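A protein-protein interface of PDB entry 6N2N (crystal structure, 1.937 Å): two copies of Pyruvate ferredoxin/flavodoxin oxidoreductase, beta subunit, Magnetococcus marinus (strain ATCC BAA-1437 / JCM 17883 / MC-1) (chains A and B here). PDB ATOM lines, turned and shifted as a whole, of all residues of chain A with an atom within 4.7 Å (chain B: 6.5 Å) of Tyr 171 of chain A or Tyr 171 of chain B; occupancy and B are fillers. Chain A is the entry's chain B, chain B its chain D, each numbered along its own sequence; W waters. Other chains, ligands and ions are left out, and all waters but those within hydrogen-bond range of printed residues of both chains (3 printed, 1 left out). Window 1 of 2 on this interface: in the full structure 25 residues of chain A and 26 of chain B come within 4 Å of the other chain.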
ATOM      1  N   GLY A 110     -15.306  -5.493  17.119  1.00  0.00           N
ATOM      2  CA  GLY A 110     -16.038  -6.556  17.785  1.00  0.00           C
ATOM      3  C   GLY A 110     -17.317  -6.980  17.091  1.00  0.00           C
ATOM      4  O   GLY A 110     -17.751  -8.121  17.277  1.00  0.00           O
ATOM      5  N   MET A 113     -16.425  -9.697  14.277  1.00  0.00           N
ATOM      6  CA  MET A 113     -15.914 -10.979  14.763  1.00  0.00           C
ATOM      7  C   MET A 113     -16.938 -12.107  14.728  1.00  0.00           C
ATOM      8  O   MET A 113     -16.601 -13.187  14.214  1.00  0.00           O
ATOM      9  CB  MET A 113     -15.360 -10.804  16.183  1.00  0.00           C
ATOM     10  CG  MET A 113     -14.076  -9.987  16.261  1.00  0.00           C
ATOM     11  SD  MET A 113     -12.763 -10.683  15.237  1.00  0.00           S
ATOM     12  CE  MET A 113     -11.395 -10.575  16.388  1.00  0.00           C
ATOM     13  N   PRO A 114     -18.171 -11.950  15.245  1.00  0.00           N
ATOM     14  CA  PRO A 114     -19.098 -13.098  15.255  1.00  0.00           C
ATOM     15  C   PRO A 114     -19.366 -13.671  13.875  1.00  0.00           C
ATOM     16  O   PRO A 114     -19.467 -14.894  13.717  1.00  0.00           O
ATOM     17  CB  PRO A 114     -20.381 -12.516  15.868  1.00  0.00           C
ATOM     18  CG  PRO A 114     -19.958 -11.302  16.587  1.00  0.00           C
ATOM     19  CD  PRO A 114     -18.789 -10.753  15.842  1.00  0.00           C
ATOM     20  N   ALA A 117     -16.548 -15.835  12.170  1.00  0.00           N
ATOM     21  CA  ALA A 117     -16.471 -17.164  12.762  1.00  0.00           C
ATOM     22  C   ALA A 117     -17.712 -17.978  12.428  1.00  0.00           C
ATOM     23  O   ALA A 117     -17.610 -19.137  12.010  1.00  0.00           O
ATOM     24  CB  ALA A 117     -16.284 -17.056  14.273  1.00  0.00           C
ATOM     25  N   ARG A 118     -18.896 -17.378  12.602  1.00  0.00           N
ATOM     26  CA  ARG A 118     -20.145 -18.078  12.322  1.00  0.00           C
ATOM     27  C   ARG A 118     -20.186 -18.585  10.887  1.00  0.00           C
ATOM     28  O   ARG A 118     -20.572 -19.732  10.637  1.00  0.00           O
ATOM     29  CB  ARG A 118     -21.332 -17.152  12.604  1.00  0.00           C
ATOM     30  CG  ARG A 118     -22.683 -17.779  12.377  1.00  0.00           C
ATOM     31  CD  ARG A 118     -23.795 -16.874  12.883  1.00  0.00           C
ATOM     32  NE  ARG A 118     -23.836 -15.592  12.182  1.00  0.00           N
ATOM     33  CZ  ARG A 118     -24.545 -15.376  11.079  1.00  0.00           C
ATOM     34  NH1 ARG A 118     -25.266 -16.362  10.557  1.00  0.00           N
ATOM     35  NH2 ARG A 118     -24.542 -14.178  10.500  1.00  0.00           N
ATOM     36  N   TYR A 167     -15.545 -16.136  23.589  1.00  0.00           N
ATOM     37  CA  TYR A 167     -16.252 -15.473  22.495  1.00  0.00           C
ATOM     38  C   TYR A 167     -16.153 -16.293  21.215  1.00  0.00           C
ATOM     39  O   TYR A 167     -17.171 -16.665  20.618  1.00  0.00           O
ATOM     40  CB  TYR A 167     -15.672 -14.078  22.255  1.00  0.00           C
ATOM     41  CG  TYR A 167     -16.208 -12.955  23.118  1.00  0.00           C
ATOM     42  CD1 TYR A 167     -16.374 -13.113  24.486  1.00  0.00           C
ATOM     43  CD2 TYR A 167     -16.512 -11.716  22.558  1.00  0.00           C
ATOM     44  CE1 TYR A 167     -16.847 -12.075  25.274  1.00  0.00           C
ATOM     45  CE2 TYR A 167     -16.980 -10.676  23.337  1.00  0.00           C
ATOM     46  CZ  TYR A 167     -17.146 -10.859  24.692  1.00  0.00           C
ATOM     47  OH  TYR A 167     -17.604  -9.819  25.471  1.00  0.00           O
ATOM     48  N   MET A 168     -14.920 -16.621  20.804  1.00  0.00           N
ATOM     49  CA  MET A 168     -14.705 -17.270  19.513  1.00  0.00           C
ATOM     50  C   MET A 168     -15.283 -18.679  19.484  1.00  0.00           C
ATOM     51  O   MET A 168     -15.776 -19.125  18.443  1.00  0.00           O
ATOM     52  CB  MET A 168     -13.214 -17.290  19.170  1.00  0.00           C
ATOM     53  CG  MET A 168     -12.690 -15.967  18.640  1.00  0.00           C
ATOM     54  SD  MET A 168     -13.515 -15.580  17.068  1.00  0.00           S
ATOM     55  CE  MET A 168     -13.063 -13.868  16.833  1.00  0.00           C
ATOM     56  N   LEU A 169     -15.223 -19.401  20.603  1.00  0.00           N
ATOM     57  CA  LEU A 169     -15.884 -20.702  20.667  1.00  0.00           C
ATOM     58  C   LEU A 169     -17.397 -20.550  20.550  1.00  0.00           C
ATOM     59  O   LEU A 169     -18.050 -21.275  19.790  1.00  0.00           O
ATOM     60  CB  LEU A 169     -15.515 -21.411  21.970  1.00  0.00           C
ATOM     61  CG  LEU A 169     -14.060 -21.867  22.116  1.00  0.00           C
ATOM     62  CD1 LEU A 169     -13.774 -22.222  23.565  1.00  0.00           C
ATOM     63  CD2 LEU A 169     -13.791 -23.049  21.201  1.00  0.00           C
ATOM     64  N   THR A 170     -17.966 -19.604  21.303  1.00  0.00           N
ATOM     65  CA  THR A 170     -19.397 -19.333  21.224  1.00  0.00           C
ATOM     66  C   THR A 170     -19.796 -18.892  19.822  1.00  0.00           C
ATOM     67  O   THR A 170     -20.851 -19.287  19.315  1.00  0.00           O
ATOM     68  CB  THR A 170     -19.772 -18.268  22.255  1.00  0.00           C
ATOM     69  OG1 THR A 170     -19.621 -18.814  23.570  1.00  0.00           O
ATOM     70  CG2 THR A 170     -21.210 -17.803  22.054  1.00  0.00           C
ATOM     71  N   TYR A 171     -18.943 -18.096  19.169  1.00  0.00           N
ATOM     72  CA  TYR A 171     -19.219 -17.616  17.821  1.00  0.00           C
ATOM     73  C   TYR A 171     -19.197 -18.730  16.784  1.00  0.00           C
ATOM     74  O   TYR A 171     -19.793 -18.575  15.711  1.00  0.00           O
ATOM     75  CB  TYR A 171     -18.201 -16.545  17.425  1.00  0.00           C
ATOM     76  CG  TYR A 171     -18.348 -15.224  18.152  1.00  0.00           C
ATOM     77  CD1 TYR A 171     -19.494 -14.925  18.884  1.00  0.00           C
ATOM     78  CD2 TYR A 171     -17.342 -14.268  18.092  1.00  0.00           C
ATOM     79  CE1 TYR A 171     -19.630 -13.712  19.537  1.00  0.00           C
ATOM     80  CE2 TYR A 171     -17.474 -13.052  18.737  1.00  0.00           C
ATOM     81  CZ  TYR A 171     -18.617 -12.778  19.455  1.00  0.00           C
ATOM     82  OH  TYR A 171     -18.744 -11.563  20.101  1.00  0.00           O
ATOM     83  N   GLY A 172     -18.522 -19.836  17.064  1.00  0.00           N
ATOM     84  CA  GLY A 172     -18.461 -20.939  16.134  1.00  0.00           C
ATOM     85  C   GLY A 172     -17.170 -21.070  15.359  1.00  0.00           C
ATOM     86  O   GLY A 172     -17.159 -21.756  14.330  1.00  0.00           O
ATOM     87  N   ALA A 173     -16.093 -20.425  15.803  1.00  0.00           N
ATOM     88  CA  ALA A 173     -14.795 -20.644  15.180  1.00  0.00           C
ATOM     89  C   ALA A 173     -14.455 -22.129  15.205  1.00  0.00           C
ATOM     90  O   ALA A 173     -14.677 -22.816  16.206  1.00  0.00           O
ATOM     91  CB  ALA A 173     -13.717 -19.836  15.900  1.00  0.00           C
ATOM     92  N   PHE B 106     -28.364  -8.369  16.611  1.00  0.00           N
ATOM     93  CA  PHE B 106     -27.186  -9.193  16.416  1.00  0.00           C
ATOM     94  C   PHE B 106     -26.563  -9.082  15.036  1.00  0.00           C
ATOM     95  O   PHE B 106     -25.489  -9.651  14.816  1.00  0.00           O
ATOM     96  CB  PHE B 106     -27.518 -10.664  16.710  1.00  0.00           C
ATOM     97  CG  PHE B 106     -27.637 -10.956  18.173  1.00  0.00           C
ATOM     98  CD1 PHE B 106     -26.515 -10.893  18.994  1.00  0.00           C
ATOM     99  CD2 PHE B 106     -28.861 -11.255  18.739  1.00  0.00           C
ATOM    100  CE1 PHE B 106     -26.616 -11.145  20.349  1.00  0.00           C
ATOM    101  CE2 PHE B 106     -28.967 -11.506  20.097  1.00  0.00           C
ATOM    102  CZ  PHE B 106     -27.849 -11.454  20.900  1.00  0.00           C
ATOM    103  N   GLY B 110     -24.700  -6.004  16.516  1.00  0.00           N
ATOM    104  CA  GLY B 110     -23.940  -7.054  17.171  1.00  0.00           C
ATOM    105  C   GLY B 110     -22.675  -6.573  17.851  1.00  0.00           C
ATOM    106  O   GLY B 110     -22.198  -7.231  18.781  1.00  0.00           O
ATOM    107  N   MET B 113     -23.627  -5.222  21.557  1.00  0.00           N
ATOM    108  CA  MET B 113     -24.107  -6.222  22.512  1.00  0.00           C
ATOM    109  C   MET B 113     -23.063  -6.661  23.534  1.00  0.00           C
ATOM    110  O   MET B 113     -23.388  -6.680  24.734  1.00  0.00           O
ATOM    111  CB  MET B 113     -24.640  -7.438  21.741  1.00  0.00           C
ATOM    112  CG  MET B 113     -25.934  -7.178  20.988  1.00  0.00           C
ATOM    113  SD  MET B 113     -27.275  -6.627  22.057  1.00  0.00           S
ATOM    114  CE  MET B 113     -28.632  -7.618  21.418  1.00  0.00           C
ATOM    115  N   PRO B 114     -21.831  -7.035  23.154  1.00  0.00           N
ATOM    116  CA  PRO B 114     -20.881  -7.521  24.170  1.00  0.00           C
ATOM    117  C   PRO B 114     -20.618  -6.526  25.283  1.00  0.00           C
ATOM    118  O   PRO B 114     -20.516  -6.920  26.450  1.00  0.00           O
ATOM    119  CB  PRO B 114     -19.604  -7.792  23.361  1.00  0.00           C
ATOM    120  CG  PRO B 114     -20.036  -7.915  21.967  1.00  0.00           C
ATOM    121  CD  PRO B 114     -21.226  -7.026  21.812  1.00  0.00           C
ATOM    122  N   HIS B 115     -20.520  -5.239  24.954  1.00  0.00           N
ATOM    123  CA  HIS B 115     -20.069  -4.260  25.934  1.00  0.00           C
ATOM    124  C   HIS B 115     -21.172  -3.854  26.900  1.00  0.00           C
ATOM    125  O   HIS B 115     -20.889  -3.600  28.075  1.00  0.00           O
ATOM    126  CB  HIS B 115     -19.473  -3.055  25.203  1.00  0.00           C
ATOM    127  CG  HIS B 115     -18.386  -3.437  24.246  1.00  0.00           C
ATOM    128  ND1 HIS B 115     -17.089  -3.683  24.651  1.00  0.00           N
ATOM    129  CD2 HIS B 115     -18.414  -3.676  22.914  1.00  0.00           C
ATOM    130  CE1 HIS B 115     -16.362  -4.033  23.605  1.00  0.00           C
ATOM    131  NE2 HIS B 115     -17.143  -4.040  22.538  1.00  0.00           N
ATOM    132  N   MET B 116     -22.429  -3.820  26.451  1.00  0.00           N
ATOM    133  CA  MET B 116     -23.536  -3.631  27.381  1.00  0.00           C
ATOM    134  C   MET B 116     -23.544  -4.719  28.441  1.00  0.00           C
ATOM    135  O   MET B 116     -23.656  -4.440  29.641  1.00  0.00           O
ATOM    136  CB  MET B 116     -24.863  -3.658  26.635  1.00  0.00           C
ATOM    137  CG  MET B 116     -25.182  -2.476  25.787  1.00  0.00           C
ATOM    138  SD  MET B 116     -26.708  -2.930  24.918  1.00  0.00           S
ATOM    139  CE  MET B 116     -26.060  -3.301  23.313  1.00  0.00           C
ATOM    140  N   ALA B 117     -23.443  -5.974  28.005  1.00  0.00           N
ATOM    141  CA  ALA B 117     -23.521  -7.096  28.933  1.00  0.00           C
ATOM    142  C   ALA B 117     -22.283  -7.165  29.818  1.00  0.00           C
ATOM    143  O   ALA B 117     -22.391  -7.334  31.039  1.00  0.00           O
ATOM    144  CB  ALA B 117     -23.699  -8.400  28.157  1.00  0.00           C
ATOM    145  N   ARG B 118     -21.100  -7.054  29.210  1.00  0.00           N
ATOM    146  CA  ARG B 118     -19.851  -7.110  29.966  1.00  0.00           C
ATOM    147  C   ARG B 118     -19.821  -6.051  31.062  1.00  0.00           C
ATOM    148  O   ARG B 118     -19.429  -6.335  32.202  1.00  0.00           O
ATOM    149  CB  ARG B 118     -18.666  -6.945  29.011  1.00  0.00           C
ATOM    150  CG  ARG B 118     -17.299  -7.017  29.664  1.00  0.00           C
ATOM    151  CD  ARG B 118     -16.193  -7.085  28.612  1.00  0.00           C
ATOM    152  NE  ARG B 118     -16.150  -5.899  27.753  1.00  0.00           N
ATOM    153  CZ  ARG B 118     -15.424  -4.815  28.021  1.00  0.00           C
ATOM    154  NH1 ARG B 118     -14.685  -4.768  29.123  1.00  0.00           N
ATOM    155  NH2 ARG B 118     -15.432  -3.780  27.190  1.00  0.00           N
ATOM    156  N   LYS B 119     -20.254  -4.834  30.747  1.00  0.00           N
ATOM    157  CA  LYS B 119     -20.271  -3.753  31.725  1.00  0.00           C
ATOM    158  C   LYS B 119     -21.440  -3.836  32.693  1.00  0.00           C
ATOM    159  O   LYS B 119     -21.514  -3.015  33.612  1.00  0.00           O
ATOM    160  CB  LYS B 119     -20.289  -2.406  31.003  1.00  0.00           C
ATOM    161  CG  LYS B 119     -19.041  -2.183  30.153  1.00  0.00           C
ATOM    162  CD  LYS B 119     -19.100  -0.884  29.385  1.00  0.00           C
ATOM    163  CE  LYS B 119     -17.856  -0.718  28.513  1.00  0.00           C
ATOM    164  NZ  LYS B 119     -17.811   0.629  27.905  1.00  0.00           N
ATOM    165  N   PRO B 161     -26.923 -20.457  11.876  1.00  0.00           N
ATOM    166  CA  PRO B 161     -27.351 -19.357  12.741  1.00  0.00           C
ATOM    167  C   PRO B 161     -26.540 -19.295  14.030  1.00  0.00           C
ATOM    168  O   PRO B 161     -25.853 -20.243  14.417  1.00  0.00           O
ATOM    169  CB  PRO B 161     -28.818 -19.691  13.031  1.00  0.00           C
ATOM    170  CG  PRO B 161     -28.880 -21.180  12.929  1.00  0.00           C
ATOM    171  CD  PRO B 161     -27.924 -21.541  11.822  1.00  0.00           C
ATOM    172  N   MET B 162     -26.624 -18.144  14.693  1.00  0.00           N
ATOM    173  CA  MET B 162     -25.972 -17.987  15.983  1.00  0.00           C
ATOM    174  C   MET B 162     -26.926 -18.331  17.125  1.00  0.00           C
ATOM    175  O   MET B 162     -28.130 -18.527  16.936  1.00  0.00           O
ATOM    176  CB  MET B 162     -25.414 -16.565  16.155  1.00  0.00           C
ATOM    177  CG  MET B 162     -26.291 -15.419  15.665  1.00  0.00           C
ATOM    178  SD  MET B 162     -27.517 -14.769  16.824  1.00  0.00           S
ATOM    179  CE  MET B 162     -26.535 -14.370  18.250  1.00  0.00           C
ATOM    180  N   LEU B 166     -26.467 -18.123  24.241  1.00  0.00           N
ATOM    181  CA  LEU B 166     -25.072 -18.456  24.501  1.00  0.00           C
ATOM    182  C   LEU B 166     -24.174 -17.233  24.359  1.00  0.00           C
ATOM    183  O   LEU B 166     -23.255 -17.045  25.161  1.00  0.00           O
ATOM    184  CB  LEU B 166     -24.616 -19.572  23.564  1.00  0.00           C
ATOM    185  CG  LEU B 166     -23.240 -20.157  23.899  1.00  0.00           C
ATOM    186  CD1 LEU B 166     -23.249 -20.833  25.259  1.00  0.00           C
ATOM    187  CD2 LEU B 166     -22.791 -21.127  22.809  1.00  0.00           C
ATOM    188  N   TYR B 167     -24.409 -16.410  23.331  1.00  0.00           N
ATOM    189  CA  TYR B 167     -23.721 -15.126  23.200  1.00  0.00           C
ATOM    190  C   TYR B 167     -23.826 -14.313  24.480  1.00  0.00           C
ATOM    191  O   TYR B 167     -22.822 -13.824  25.012  1.00  0.00           O
ATOM    192  CB  TYR B 167     -24.324 -14.315  22.049  1.00  0.00           C
ATOM    193  CG  TYR B 167     -23.775 -14.582  20.670  1.00  0.00           C
ATOM    194  CD1 TYR B 167     -23.551 -15.877  20.222  1.00  0.00           C
ATOM    195  CD2 TYR B 167     -23.519 -13.529  19.795  1.00  0.00           C
ATOM    196  CE1 TYR B 167     -23.068 -16.116  18.950  1.00  0.00           C
ATOM    197  CE2 TYR B 167     -23.035 -13.762  18.519  1.00  0.00           C
ATOM    198  CZ  TYR B 167     -22.809 -15.056  18.104  1.00  0.00           C
ATOM    199  OH  TYR B 167     -22.338 -15.295  16.833  1.00  0.00           O
ATOM    200  N   MET B 168     -25.051 -14.128  24.967  1.00  0.00           N
ATOM    201  CA  MET B 168     -25.269 -13.216  26.079  1.00  0.00           C
ATOM    202  C   MET B 168     -24.681 -13.770  27.371  1.00  0.00           C
ATOM    203  O   MET B 168     -24.155 -13.009  28.192  1.00  0.00           O
ATOM    204  CB  MET B 168     -26.762 -12.931  26.218  1.00  0.00           C
ATOM    205  CG  MET B 168     -27.311 -12.065  25.081  1.00  0.00           C
ATOM    206  SD  MET B 168     -26.554 -10.429  24.957  1.00  0.00           S
ATOM    207  CE  MET B 168     -26.452 -10.032  26.669  1.00  0.00           C
ATOM    208  N   LEU B 169     -24.745 -15.091  27.563  1.00  0.00           N
ATOM    209  CA  LEU B 169     -24.076 -15.701  28.710  1.00  0.00           C
ATOM    210  C   LEU B 169     -22.566 -15.512  28.611  1.00  0.00           C
ATOM    211  O   LEU B 169     -21.906 -15.147  29.589  1.00  0.00           O
ATOM    212  CB  LEU B 169     -24.429 -17.189  28.804  1.00  0.00           C
ATOM    213  CG  LEU B 169     -25.879 -17.534  29.178  1.00  0.00           C
ATOM    214  CD1 LEU B 169     -26.176 -18.998  28.891  1.00  0.00           C
ATOM    215  CD2 LEU B 169     -26.147 -17.214  30.641  1.00  0.00           C
ATOM    216  N   THR B 170     -22.007 -15.761  27.425  1.00  0.00           N
ATOM    217  CA  THR B 170     -20.582 -15.545  27.200  1.00  0.00           C
ATOM    218  C   THR B 170     -20.197 -14.086  27.411  1.00  0.00           C
ATOM    219  O   THR B 170     -19.124 -13.790  27.955  1.00  0.00           O
ATOM    220  CB  THR B 170     -20.219 -16.004  25.787  1.00  0.00           C
ATOM    221  OG1 THR B 170     -20.327 -17.430  25.716  1.00  0.00           O
ATOM    222  CG2 THR B 170     -18.810 -15.583  25.406  1.00  0.00           C
ATOM    223  N   TYR B 171     -21.061 -13.158  26.992  1.00  0.00           N
ATOM    224  CA  TYR B 171     -20.781 -11.734  27.141  1.00  0.00           C
ATOM    225  C   TYR B 171     -20.808 -11.274  28.593  1.00  0.00           C
ATOM    226  O   TYR B 171     -20.228 -10.229  28.904  1.00  0.00           O
ATOM    227  CB  TYR B 171     -21.785 -10.901  26.338  1.00  0.00           C
ATOM    228  CG  TYR B 171     -21.643 -10.993  24.830  1.00  0.00           C
ATOM    229  CD1 TYR B 171     -20.507 -11.540  24.243  1.00  0.00           C
ATOM    230  CD2 TYR B 171     -22.663 -10.537  23.995  1.00  0.00           C
ATOM    231  CE1 TYR B 171     -20.385 -11.617  22.866  1.00  0.00           C
ATOM    232  CE2 TYR B 171     -22.550 -10.606  22.622  1.00  0.00           C
ATOM    233  CZ  TYR B 171     -21.415 -11.147  22.061  1.00  0.00           C
ATOM    234  OH  TYR B 171     -21.312 -11.209  20.690  1.00  0.00           O
ATOM    235  N   GLY B 172     -21.473 -12.006  29.478  1.00  0.00           N
ATOM    236  CA  GLY B 172     -21.550 -11.622  30.872  1.00  0.00           C
ATOM    237  C   GLY B 172     -22.866 -11.022  31.329  1.00  0.00           C
ATOM    238  O   GLY B 172     -22.892 -10.367  32.376  1.00  0.00           O
ATOM    239  N   ALA B 173     -23.946 -11.198  30.573  1.00  0.00           N
ATOM    240  CA  ALA B 173     -25.255 -10.792  31.064  1.00  0.00           C
ATOM    241  C   ALA B 173     -25.548 -11.483  32.391  1.00  0.00           C
ATOM    242  O   ALA B 173     -25.294 -12.678  32.552  1.00  0.00           O
ATOM    243  CB  ALA B 173     -26.338 -11.136  30.040  1.00  0.00           C
ATOM    244  N   MET B 241     -25.114 -22.412  30.300  1.00  0.00           N
ATOM    245  CA  MET B 241     -24.611 -22.517  28.935  1.00  0.00           C
ATOM    246  C   MET B 241     -24.997 -23.848  28.298  1.00  0.00           C
ATOM    247  O   MET B 241     -25.263 -23.903  27.091  1.00  0.00           O
ATOM    248  CB  MET B 241     -23.090 -22.329  28.919  1.00  0.00           C
ATOM    249  CG  MET B 241     -22.622 -20.929  29.325  1.00  0.00           C
ATOM    250  SD  MET B 241     -20.813 -20.739  29.278  1.00  0.00           S
ATOM    251  CE  MET B 241     -20.652 -18.958  29.399  1.00  0.00           C
HETATM  252  O   HOH W   1     -22.321 -17.623  16.053  1.00  0.00           O
HETATM  253  O   HOH W   2     -17.664 -10.135  27.906  1.00  0.00           O
HETATM  254  O   HOH W   3     -23.060 -13.924  14.585  1.00  0.00           O
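The side-chain hydroxyl of Thr 170 of chain B lies within hydrogen-bond range of the side-chain hydroxyl of Thr 170 of chain A, at 2.6 Å.
The side-chain hydroxyl (OH) of Tyr 171 of chain B is in hydrogen-bond range of the side-chain hydroxyl (OH) of Tyr 171 of chain A (2.7 Å).
Of the 20 printed residues of chain B, 7 touch a printed residue of chain A.
Printed residues of chain B that touch a printed residue of chain A: Pro 114, Pro 161, Met 162, Leu 166, Tyr 167, Thr 170 and Tyr 171.
Hydrophobic or aromatic side chains of chain B that line the printed part of chain A: Pro 114, Met 162, Leu 166, Tyr 167 and Tyr 171.
Along chain B the printed residues that touch a printed residue of chain A span positions 114 to 171.
Of the 12 printed residues of chain A, 5 touch a printed residue of chain B.
Printed residues of chain A that touch a printed residue of chain B: Pro 114, Arg 118, Tyr 167, Thr 170 and Tyr 171.
Hydrophobic or aromatic side chains of chain A that line the printed part of chain B: Pro 114, Tyr 167 and Tyr 171.
Among the printed residues, 11 pairs touch across the chains.
Among the printed residues, no Asp or Glu carboxylate lies within 4 Å of a Lys or Arg side-chain nitrogen of the other chain.
Water W1 lies within hydrogen-bond range of the side-chain hydroxyl of Tyr 167 of chain B and the backbone carbonyl oxygen of Tyr 171 of chain A.
Water W2 lies within hydrogen-bond range of the side-chain hydroxyl of Tyr 167 of chain A and the backbone carbonyl oxygen of Tyr 171 of chain B.
Water W3 bridges the side-chain hydroxyl (OH) of Tyr 167 of chain B and the guanidinium group (NE) of Arg 118 of chain A.
O of Tyr 171 of chain A sits close to N of Arg 118 of chain A.
N of Arg 118 of chain B is in hydrogen-bond range of O of Tyr 171 of chain B, at 3.3 Å.
O of Leu 166 of chain B is in hydrogen-bond range of OG1 of Thr 170 of chain B (3.0 Å).
Tyr 167 of chain A touches Thr 170 of chain B, and with the chains exchanged Thr 170 of chain A touches Tyr 167 of chain B.
Tyr 167 of chain A touches Tyr 171 of chain B, and with the chains exchanged Tyr 171 of chain A touches Tyr 167 of chain B.
Thr 170 of chain A touches its own counterpart, Thr 170 of chain B.
Tyr 171 of chain B touches its own counterpart, Tyr 171 of chain A.
Positions printed for both chains: 110, 113, 114, 117, 118, 167, 168, 169, 170, 171, 172 and 173.
Of the 11 pairs that touch across the chains among the printed residues, 8 have their exchanged pair printed and touching as well.
Among the printed residues, pairs that only touch across the chains: Tyr 171 of chain A with Tyr 167 of chain B (3.4 Å), Tyr 167 of chain A with Tyr 171 of chain B (3.5 Å), Pro 114 of chain A with Tyr 167 of chain B (3.5 Å), Thr 170 of chain A with Tyr 167 of chain B (3.5 Å), Tyr 167 of chain A with Pro 114 of chain B (3.5 Å), Tyr 167 of chain A with Thr 170 of chain B (3.6 Å), Arg 118 of chain A with Met 162 of chain B (3.6 Å), Thr 170 of chain A with Leu 166 of chain B (3.6 Å) and Arg 118 of chain A with Pro 161 of chain B (3.8 Å).
Tyr 171 of chain A touches just these residues of chain B: Tyr 167 (3.4 Å) and Tyr 171 (2.7 Å).
Of chain A, only Tyr 167 and Tyr 171 come within 4 Å of Tyr 171 of chain B.
Printed residues of chain A within 4 Å of Thr 170 of chain B: Tyr 167 (3.6 Å) and Thr 170 (2.6 Å).
Of the printed residues of chain A, Leu 166 of chain B touches Thr 170.
Leu 169 of chain B touches none of the printed residues of chain A.
Arg 118 of chain B touches none of the printed residues of chain A.
The nearest residue of chain A that does not touch Tyr 171 of chain B is Pro 114 of chain A (4.3 Å).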
